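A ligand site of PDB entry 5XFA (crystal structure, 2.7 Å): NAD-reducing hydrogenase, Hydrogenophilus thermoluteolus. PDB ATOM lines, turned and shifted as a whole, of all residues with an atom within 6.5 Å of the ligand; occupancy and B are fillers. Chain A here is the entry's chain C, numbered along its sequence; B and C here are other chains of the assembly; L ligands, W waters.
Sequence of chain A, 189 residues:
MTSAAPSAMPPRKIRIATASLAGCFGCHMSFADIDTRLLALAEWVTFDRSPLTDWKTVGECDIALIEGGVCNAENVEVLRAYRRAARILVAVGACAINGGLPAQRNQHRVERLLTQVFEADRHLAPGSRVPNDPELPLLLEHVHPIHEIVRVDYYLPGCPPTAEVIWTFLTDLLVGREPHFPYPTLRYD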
ATOM      1  N   SER A  20       4.696  -4.081   3.011  1.00  0.00           N
ATOM      2  CA  SER A  20       3.265  -3.785   3.086  1.00  0.00           C
ATOM      3  C   SER A  20       2.490  -4.831   2.315  1.00  0.00           C
ATOM      4  O   SER A  20       2.703  -5.029   1.131  1.00  0.00           O
ATOM      5  CB  SER A  20       2.960  -2.403   2.523  1.00  0.00           C
ATOM      6  OG  SER A  20       1.566  -2.145   2.585  1.00  0.00           O
ATOM      7  N   ALA A  22      -1.773  -6.176   2.505  1.00  0.00           N
ATOM      8  CA  ALA A  22      -2.981  -5.404   2.250  1.00  0.00           C
ATOM      9  C   ALA A  22      -3.032  -4.137   3.136  1.00  0.00           C
ATOM     10  O   ALA A  22      -4.072  -3.846   3.779  1.00  0.00           O
ATOM     11  CB  ALA A  22      -4.206  -6.263   2.469  1.00  0.00           C
ATOM     12  N   GLY A  23      -1.954  -3.363   3.122  1.00  0.00           N
ATOM     13  CA  GLY A  23      -1.864  -2.179   3.959  1.00  0.00           C
ATOM     14  C   GLY A  23      -2.189  -0.932   3.182  1.00  0.00           C
ATOM     15  O   GLY A  23      -2.407  -0.992   1.964  1.00  0.00           O
ATOM     16  N   CYS A  24      -2.227   0.210   3.882  1.00  0.00           N
ATOM     17  CA  CYS A  24      -2.412   1.498   3.223  1.00  0.00           C
ATOM     18  C   CYS A  24      -1.106   2.328   3.128  1.00  0.00           C
ATOM     19  O   CYS A  24      -1.128   3.479   2.686  1.00  0.00           O
ATOM     20  CB  CYS A  24      -3.486   2.281   3.934  1.00  0.00           C
ATOM     21  SG  CYS A  24      -2.917   3.167   5.398  1.00  0.00           S
ATOM     22  N   PHE A  25       0.032   1.735   3.504  1.00  0.00           N
ATOM     23  CA  PHE A  25       1.311   2.442   3.581  1.00  0.00           C
ATOM     24  C   PHE A  25       1.362   3.321   4.826  1.00  0.00           C
ATOM     25  O   PHE A  25       2.412   3.998   5.080  1.00  0.00           O
ATOM     26  CB  PHE A  25       1.564   3.279   2.347  1.00  0.00           C
ATOM     27  CG  PHE A  25       3.034   3.509   2.057  1.00  0.00           C
ATOM     28  CD1 PHE A  25       3.848   2.451   1.668  1.00  0.00           C
ATOM     29  CD2 PHE A  25       3.572   4.792   2.131  1.00  0.00           C
ATOM     30  CE1 PHE A  25       5.189   2.673   1.389  1.00  0.00           C
ATOM     31  CE2 PHE A  25       4.897   4.992   1.852  1.00  0.00           C
ATOM     32  CZ  PHE A  25       5.714   3.939   1.487  1.00  0.00           C
ATOM     33  N   GLY A  26       0.295   3.282   5.635  1.00  0.00           N
ATOM     34  CA  GLY A  26       0.160   4.245   6.719  1.00  0.00           C
ATOM     35  C   GLY A  26       1.060   3.928   7.875  1.00  0.00           C
ATOM     36  O   GLY A  26       1.438   4.835   8.667  1.00  0.00           O
ATOM     37  N   CYS A  27       1.410   2.651   7.984  1.00  0.00           N
ATOM     38  CA  CYS A  27       2.238   2.255   9.110  1.00  0.00           C
ATOM     39  C   CYS A  27       3.646   2.669   8.807  1.00  0.00           C
ATOM     40  O   CYS A  27       4.380   3.092   9.703  1.00  0.00           O
ATOM     41  CB  CYS A  27       2.081   0.780   9.483  1.00  0.00           C
ATOM     42  SG  CYS A  27       0.449   0.392  10.276  1.00  0.00           S
ATOM     43  N   HIS A  28       4.013   2.638   7.523  1.00  0.00           N
ATOM     44  CA  HIS A  28       5.338   3.090   7.132  1.00  0.00           C
ATOM     45  C   HIS A  28       5.443   4.601   7.302  1.00  0.00           C
ATOM     46  O   HIS A  28       6.536   5.092   7.577  1.00  0.00           O
ATOM     47  CB  HIS A  28       5.651   2.700   5.724  1.00  0.00           C
ATOM     48  CG  HIS A  28       5.984   1.242   5.563  1.00  0.00           C
ATOM     49  ND1 HIS A  28       5.038   0.239   5.690  1.00  0.00           N
ATOM     50  CD2 HIS A  28       7.141   0.624   5.219  1.00  0.00           C
ATOM     51  CE1 HIS A  28       5.612  -0.922   5.473  1.00  0.00           C
ATOM     52  NE2 HIS A  28       6.891  -0.723   5.175  1.00  0.00           N
ATOM     53  N   GLU A  67       3.357  -4.457   7.584  1.00  0.00           N
ATOM     54  CA  GLU A  67       2.051  -3.793   7.754  1.00  0.00           C
ATOM     55  C   GLU A  67       1.070  -4.481   6.829  1.00  0.00           C
ATOM     56  O   GLU A  67       1.482  -5.105   5.834  1.00  0.00           O
ATOM     57  CB  GLU A  67       2.121  -2.312   7.430  1.00  0.00           C
ATOM     58  CG  GLU A  67       2.115  -1.960   5.930  1.00  0.00           C
ATOM     59  CD  GLU A  67       1.650  -0.530   5.636  1.00  0.00           C
ATOM     60  OE1 GLU A  67       1.057  -0.336   4.545  1.00  0.00           O
ATOM     61  OE2 GLU A  67       1.827   0.372   6.487  1.00  0.00           O
ATOM     62  N   GLY A  68      -0.217  -4.388   7.158  1.00  0.00           N
ATOM     63  CA  GLY A  68      -1.250  -4.838   6.247  1.00  0.00           C
ATOM     64  C   GLY A  68      -1.696  -6.259   6.472  1.00  0.00           C
ATOM     65  O   GLY A  68      -0.912  -7.070   6.968  1.00  0.00           O
ATOM     66  N   GLY A  69      -2.945  -6.556   6.101  1.00  0.00           N
ATOM     67  CA  GLY A  69      -3.496  -7.919   6.207  1.00  0.00           C
ATOM     68  C   GLY A  69      -3.025  -8.776   5.047  1.00  0.00           C
ATOM     69  O   GLY A  69      -2.174  -8.346   4.286  1.00  0.00           O
ATOM     70  N   VAL A  92       2.657  -5.056  12.443  1.00  0.00           N
ATOM     71  CA  VAL A  92       2.533  -3.645  12.668  1.00  0.00           C
ATOM     72  C   VAL A  92       1.165  -3.203  12.202  1.00  0.00           C
ATOM     73  O   VAL A  92       0.694  -3.597  11.119  1.00  0.00           O
ATOM     74  CB  VAL A  92       3.626  -2.919  11.850  1.00  0.00           C
ATOM     75  CG1 VAL A  92       3.500  -1.425  11.960  1.00  0.00           C
ATOM     76  CG2 VAL A  92       4.982  -3.351  12.324  1.00  0.00           C
ATOM     77  N   GLY A  93       0.506  -2.385  12.998  1.00  0.00           N
ATOM     78  CA  GLY A  93      -0.813  -1.858  12.622  1.00  0.00           C
ATOM     79  C   GLY A  93      -2.013  -2.789  12.763  1.00  0.00           C
ATOM     80  O   GLY A  93      -1.895  -4.009  12.706  1.00  0.00           O
ATOM     81  N   ALA A  94      -3.188  -2.181  12.886  1.00  0.00           N
ATOM     82  CA  ALA A  94      -4.463  -2.901  12.936  1.00  0.00           C
ATOM     83  C   ALA A  94      -4.683  -3.919  11.823  1.00  0.00           C
ATOM     84  O   ALA A  94      -5.220  -4.991  12.034  1.00  0.00           O
ATOM     85  CB  ALA A  94      -5.591  -1.907  12.884  1.00  0.00           C
ATOM     86  N   CYS A  95      -4.302  -3.539  10.614  1.00  0.00           N
ATOM     87  CA  CYS A  95      -4.458  -4.410   9.449  1.00  0.00           C
ATOM     88  C   CYS A  95      -3.809  -5.768   9.702  1.00  0.00           C
ATOM     89  O   CYS A  95      -4.436  -6.801   9.494  1.00  0.00           O
ATOM     90  CB  CYS A  95      -3.789  -3.780   8.210  1.00  0.00           C
ATOM     91  SG  CYS A  95      -4.737  -2.487   7.386  1.00  0.00           S
ATOM     92  N   ALA A  96      -2.537  -5.740  10.089  1.00  0.00           N
ATOM     93  CA  ALA A  96      -1.750  -6.971  10.200  1.00  0.00           C
ATOM     94  C   ALA A  96      -2.149  -7.731  11.443  1.00  0.00           C
ATOM     95  O   ALA A  96      -2.065  -8.970  11.498  1.00  0.00           O
ATOM     96  CB  ALA A  96      -0.255  -6.647  10.218  1.00  0.00           C
ATOM     97  N   GLY A 100      -7.840  -5.522  10.075  1.00  0.00           N
ATOM     98  CA  GLY A 100      -8.193  -4.107   9.897  1.00  0.00           C
ATOM     99  C   GLY A 100      -9.509  -3.829   9.185  1.00  0.00           C
ATOM    100  O   GLY A 100     -10.240  -4.735   8.789  1.00  0.00           O
ATOM    101  N   LEU A 101      -9.782  -2.549   8.989  1.00  0.00           N
ATOM    102  CA  LEU A 101     -10.903  -2.099   8.145  1.00  0.00           C
ATOM    103  C   LEU A 101     -11.058  -2.779   6.751  1.00  0.00           C
ATOM    104  O   LEU A 101     -12.170  -2.912   6.242  1.00  0.00           O
ATOM    105  CB  LEU A 101     -10.839  -0.570   7.971  1.00  0.00           C
ATOM    106  CG  LEU A 101     -11.782   0.307   8.788  1.00  0.00           C
ATOM    107  CD1 LEU A 101     -11.998  -0.194  10.210  1.00  0.00           C
ATOM    108  CD2 LEU A 101     -11.273   1.729   8.813  1.00  0.00           C
ATOM    109  N   PRO A 102      -9.960  -3.169   6.101  1.00  0.00           N
ATOM    110  CA  PRO A 102     -10.166  -3.937   4.874  1.00  0.00           C
ATOM    111  C   PRO A 102     -10.941  -5.200   5.109  1.00  0.00           C
ATOM    112  O   PRO A 102     -11.714  -5.630   4.262  1.00  0.00           O
ATOM    113  CB  PRO A 102      -8.746  -4.285   4.434  1.00  0.00           C
ATOM    114  CG  PRO A 102      -7.936  -3.128   4.921  1.00  0.00           C
ATOM    115  CD  PRO A 102      -8.581  -2.648   6.199  1.00  0.00           C
ATOM    116  N   GLY A 158      -2.414  -0.080  16.611  1.00  0.00           N
ATOM    117  CA  GLY A 158      -2.694   1.272  16.124  1.00  0.00           C
ATOM    118  C   GLY A 158      -3.041   1.252  14.654  1.00  0.00           C
ATOM    119  O   GLY A 158      -2.781   0.277  13.947  1.00  0.00           O
ATOM    120  N   CYS A 159      -3.665   2.315  14.193  1.00  0.00           N
ATOM    121  CA  CYS A 159      -4.018   2.416  12.786  1.00  0.00           C
ATOM    122  C   CYS A 159      -3.777   3.836  12.394  1.00  0.00           C
ATOM    123  O   CYS A 159      -4.728   4.568  12.181  1.00  0.00           O
ATOM    124  CB  CYS A 159      -5.496   2.000  12.572  1.00  0.00           C
ATOM    125  SG  CYS A 159      -5.949   1.779  10.833  1.00  0.00           S
ATOM    126  N   PRO A 160      -2.507   4.255  12.407  1.00  0.00           N
ATOM    127  CA  PRO A 160      -1.370   3.376  12.730  1.00  0.00           C
ATOM    128  C   PRO A 160      -0.823   3.536  14.152  1.00  0.00           C
ATOM    129  O   PRO A 160      -1.139   4.500  14.823  1.00  0.00           O
ATOM    130  CB  PRO A 160      -0.294   3.883  11.767  1.00  0.00           C
ATOM    131  CG  PRO A 160      -0.533   5.333  11.803  1.00  0.00           C
ATOM    132  CD  PRO A 160      -2.037   5.491  11.762  1.00  0.00           C
ATOM    133  N   PRO A 161       0.038   2.602  14.584  1.00  0.00           N
ATOM    134  CA  PRO A 161       0.795   2.825  15.810  1.00  0.00           C
ATOM    135  C   PRO A 161       1.368   4.189  15.842  1.00  0.00           C
ATOM    136  O   PRO A 161       1.709   4.687  14.786  1.00  0.00           O
ATOM    137  CB  PRO A 161       1.933   1.816  15.703  1.00  0.00           C
ATOM    138  CG  PRO A 161       1.610   0.924  14.546  1.00  0.00           C
ATOM    139  CD  PRO A 161       0.218   1.223  14.100  1.00  0.00           C
ATOM    140  N   ARG B  58      -8.656  -3.815  -2.740  1.00  0.00           N
ATOM    141  CA  ARG B  58      -9.316  -4.086  -1.460  1.00  0.00           C
ATOM    142  C   ARG B  58     -10.835  -3.934  -1.505  1.00  0.00           C
ATOM    143  O   ARG B  58     -11.550  -4.550  -0.715  1.00  0.00           O
ATOM    144  CB  ARG B  58      -8.723  -3.196  -0.388  1.00  0.00           C
ATOM    145  CG  ARG B  58      -7.282  -3.594  -0.042  1.00  0.00           C
ATOM    146  CD  ARG B  58      -6.545  -2.500   0.714  1.00  0.00           C
ATOM    147  NE  ARG B  58      -6.448  -1.278  -0.100  1.00  0.00           N
ATOM    148  CZ  ARG B  58      -6.273  -0.039   0.378  1.00  0.00           C
ATOM    149  NH1 ARG B  58      -6.175   0.185   1.686  1.00  0.00           N
ATOM    150  NH2 ARG B  58      -6.222   0.978  -0.477  1.00  0.00           N
ATOM    151  N   ARG B  78      -8.724   5.250   5.038  1.00  0.00           N
ATOM    152  CA  ARG B  78      -7.777   4.146   5.144  1.00  0.00           C
ATOM    153  C   ARG B  78      -7.309   3.643   3.782  1.00  0.00           C
ATOM    154  O   ARG B  78      -6.538   2.694   3.732  1.00  0.00           O
ATOM    155  CB  ARG B  78      -8.360   2.986   5.981  1.00  0.00           C
ATOM    156  CG  ARG B  78      -7.965   2.997   7.434  1.00  0.00           C
ATOM    157  CD  ARG B  78      -8.453   4.219   8.189  1.00  0.00           C
ATOM    158  NE  ARG B  78      -7.856   4.278   9.528  1.00  0.00           N
ATOM    159  CZ  ARG B  78      -8.295   5.012  10.541  1.00  0.00           C
ATOM    160  NH1 ARG B  78      -9.352   5.782  10.422  1.00  0.00           N
ATOM    161  NH2 ARG B  78      -7.652   4.975  11.698  1.00  0.00           N
ATOM    162  N   LEU B  79      -7.816   4.219   2.686  1.00  0.00           N
ATOM    163  CA  LEU B  79      -7.260   3.988   1.338  1.00  0.00           C
ATOM    164  C   LEU B  79      -5.756   4.226   1.284  1.00  0.00           C
ATOM    165  O   LEU B  79      -5.037   3.503   0.595  1.00  0.00           O
ATOM    166  CB  LEU B  79      -7.888   4.917   0.278  1.00  0.00           C
ATOM    167  CG  LEU B  79      -9.283   4.683  -0.335  1.00  0.00           C
ATOM    168  CD1 LEU B  79      -9.365   5.254  -1.746  1.00  0.00           C
ATOM    169  CD2 LEU B  79      -9.651   3.223  -0.336  1.00  0.00           C
ATOM    170  N   CYS B  80      -5.285   5.250   1.989  1.00  0.00           N
ATOM    171  CA  CYS B  80      -3.932   5.641   1.870  1.00  0.00           C
ATOM    172  C   CYS B  80      -3.427   6.337   3.103  1.00  0.00           C
ATOM    173  O   CYS B  80      -4.108   7.147   3.708  1.00  0.00           O
ATOM    174  CB  CYS B  80      -3.778   6.555   0.634  1.00  0.00           C
ATOM    175  SG  CYS B  80      -2.105   7.173   0.410  1.00  0.00           S
ATOM    176  N   GLY B  81      -2.175   6.050   3.430  1.00  0.00           N
ATOM    177  CA  GLY B  81      -1.502   6.599   4.605  1.00  0.00           C
ATOM    178  C   GLY B  81      -0.606   7.759   4.286  1.00  0.00           C
ATOM    179  O   GLY B  81       0.006   8.322   5.206  1.00  0.00           O
ATOM    180  N   ILE B 182      -1.944  10.879  11.128  1.00  0.00           N
ATOM    181  CA  ILE B 182      -2.427   9.940  10.134  1.00  0.00           C
ATOM    182  C   ILE B 182      -3.783   9.386  10.561  1.00  0.00           C
ATOM    183  O   ILE B 182      -3.888   8.679  11.535  1.00  0.00           O
ATOM    184  CB  ILE B 182      -1.458   8.767   9.936  1.00  0.00           C
ATOM    185  CG1 ILE B 182      -0.056   9.274   9.664  1.00  0.00           C
ATOM    186  CG2 ILE B 182      -1.897   7.929   8.760  1.00  0.00           C
ATOM    187  CD1 ILE B 182       0.964   8.151   9.535  1.00  0.00           C
ATOM    188  N   HIS B 183      -4.817   9.723   9.798  1.00  0.00           N
ATOM    189  CA  HIS B 183      -6.164   9.237  10.014  1.00  0.00           C
ATOM    190  C   HIS B 183      -6.879   9.942  11.167  1.00  0.00           C
ATOM    191  O   HIS B 183      -7.193   9.317  12.162  1.00  0.00           O
ATOM    192  CB  HIS B 183      -6.191   7.723  10.255  1.00  0.00           C
ATOM    193  CG  HIS B 183      -5.671   6.892   9.116  1.00  0.00           C
ATOM    194  ND1 HIS B 183      -5.995   7.130   7.805  1.00  0.00           N
ATOM    195  CD2 HIS B 183      -4.885   5.788   9.121  1.00  0.00           C
ATOM    196  CE1 HIS B 183      -5.409   6.226   7.038  1.00  0.00           C
ATOM    197  NE2 HIS B 183      -4.733   5.405   7.811  1.00  0.00           N
ATOM    198  N   PRO C 106     -10.571   1.269  14.464  1.00  0.00           N
ATOM    199  CA  PRO C 106     -10.246   2.440  13.618  1.00  0.00           C
ATOM    200  C   PRO C 106     -11.396   3.136  12.868  1.00  0.00           C
ATOM    201  O   PRO C 106     -11.220   4.249  12.386  1.00  0.00           O
ATOM    202  CB  PRO C 106      -9.264   1.867  12.585  1.00  0.00           C
ATOM    203  CG  PRO C 106      -8.608   0.740  13.288  1.00  0.00           C
ATOM    204  CD  PRO C 106      -9.696   0.135  14.132  1.00  0.00           C
HETATM  205 FE1  LIG L   1      -3.795  -0.604   8.201  1.00  0.00          FE
HETATM  206 FE2  LIG L   1      -4.082   1.639   9.484  1.00  0.00          FE
HETATM  207 FE3  LIG L   1      -2.787   1.687   7.111  1.00  0.00          FE
HETATM  208 FE4  LIG L   1      -1.464   0.701   9.037  1.00  0.00          FE
HETATM  209  S1  LIG L   1      -2.121   2.817   8.907  1.00  0.00           S
HETATM  210  S2  LIG L   1      -1.841  -0.365   7.056  1.00  0.00           S
HETATM  211  S3  LIG L   1      -3.146  -0.190  10.322  1.00  0.00           S
HETATM  212  S4  LIG L   1      -4.947   1.160   7.436  1.00  0.00           S
HETATM  213  O   HOH W   1      -6.589  -0.476   9.289  1.00  0.00           O
HETATM  214  O   HOH W   2      -0.534  -2.072   8.869  1.00  0.00           O
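The side-chain sulfur (SG) of Cys 95 is bound to an iron atom (FE1) of the ligand (2.3 Å). The side-chain sulfur (SG) of Cys 159 binds an iron atom (FE2) of the ligand (2.3 Å). The backbone NH (N) of Ala 94 sits close to a sulfur (S3) of the ligand (3.2 Å). The side-chain sulfur of Cys 27 is bound to an iron atom (FE4) of the ligand, 2.3 Å away. The side-chain sulfur (SG) of Cys 24 is bound to an iron atom (FE3) of the ligand, at 2.3 Å. A sulfur (S2) of the ligand sits close to the backbone NH (N) of Cys 24. A sulfur (S3) of the ligand lies close to the backbone NH (N) of Cys 95 (3.6 Å). S1 of the ligand sits close to N of Cys 27.
The backbone NH (N) of Ala 94 lies within hydrogen-bond range of the backbone carbonyl oxygen (O) of Gly 158 (2.7 Å). NH1 of Arg 78 of chain B is in hydrogen-bond range of O of Pro 106 of chain C. The backbone NH of Cys 27 lies within hydrogen-bond range of the side-chain carboxylate of Glu 67, at 2.8 Å. SG of Cys 24 lies close to NE2 of His 183 of chain B. The side-chain sulfur (SG) of Cys 24 lies close to the backbone NH (N) of Gly 26 (3.2 Å). The side-chain carboxylate (OE2) of Glu 67 is in hydrogen-bond range of a ring nitrogen (ND1) of His 28. The guanidinium group (NH1) of Arg 58 of chain B lies within hydrogen-bond range of the backbone carbonyl oxygen (O) of Arg 78 of chain B (3.3 Å). The backbone NH (N) of Cys 24 lies within hydrogen-bond range of the side-chain carboxylate (OE1) of Glu 67 (3.4 Å).
The side-chain carboxylate of Glu 67 sits close to a sulfur (S2) of the ligand (3.8 Å). The backbone carbonyl oxygen (O) of Gly 158 sits close to a sulfur (S3) of the ligand (3.7 Å). Residues that only touch the ligand: Gly 26 (3.5 Å), Arg 78 of chain B (3.5 Å), Pro 160 (3.6 Å), Gly 23 (3.6 Å), Gly 93 (3.7 Å) and His 183 of chain B (3.8 Å). Within 4 Å of the ligand: Gly 23, Cys 24, Gly 26, Cys 27, Glu 67, Gly 93, Ala 94, Cys 95, Gly 158, Cys 159, Pro 160, Arg 78 of chain B and His 183 of chain B. Along chain A the residues within 4 Å of the ligand span positions 23 to 160.
Water W2 lies within hydrogen-bond range of a sulfur (S2) of the ligand (2.8 Å), the backbone NH (N) of Gly 68 (2.9 Å) and the backbone carbonyl oxygen (O) of Val 92 (3.0 Å).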
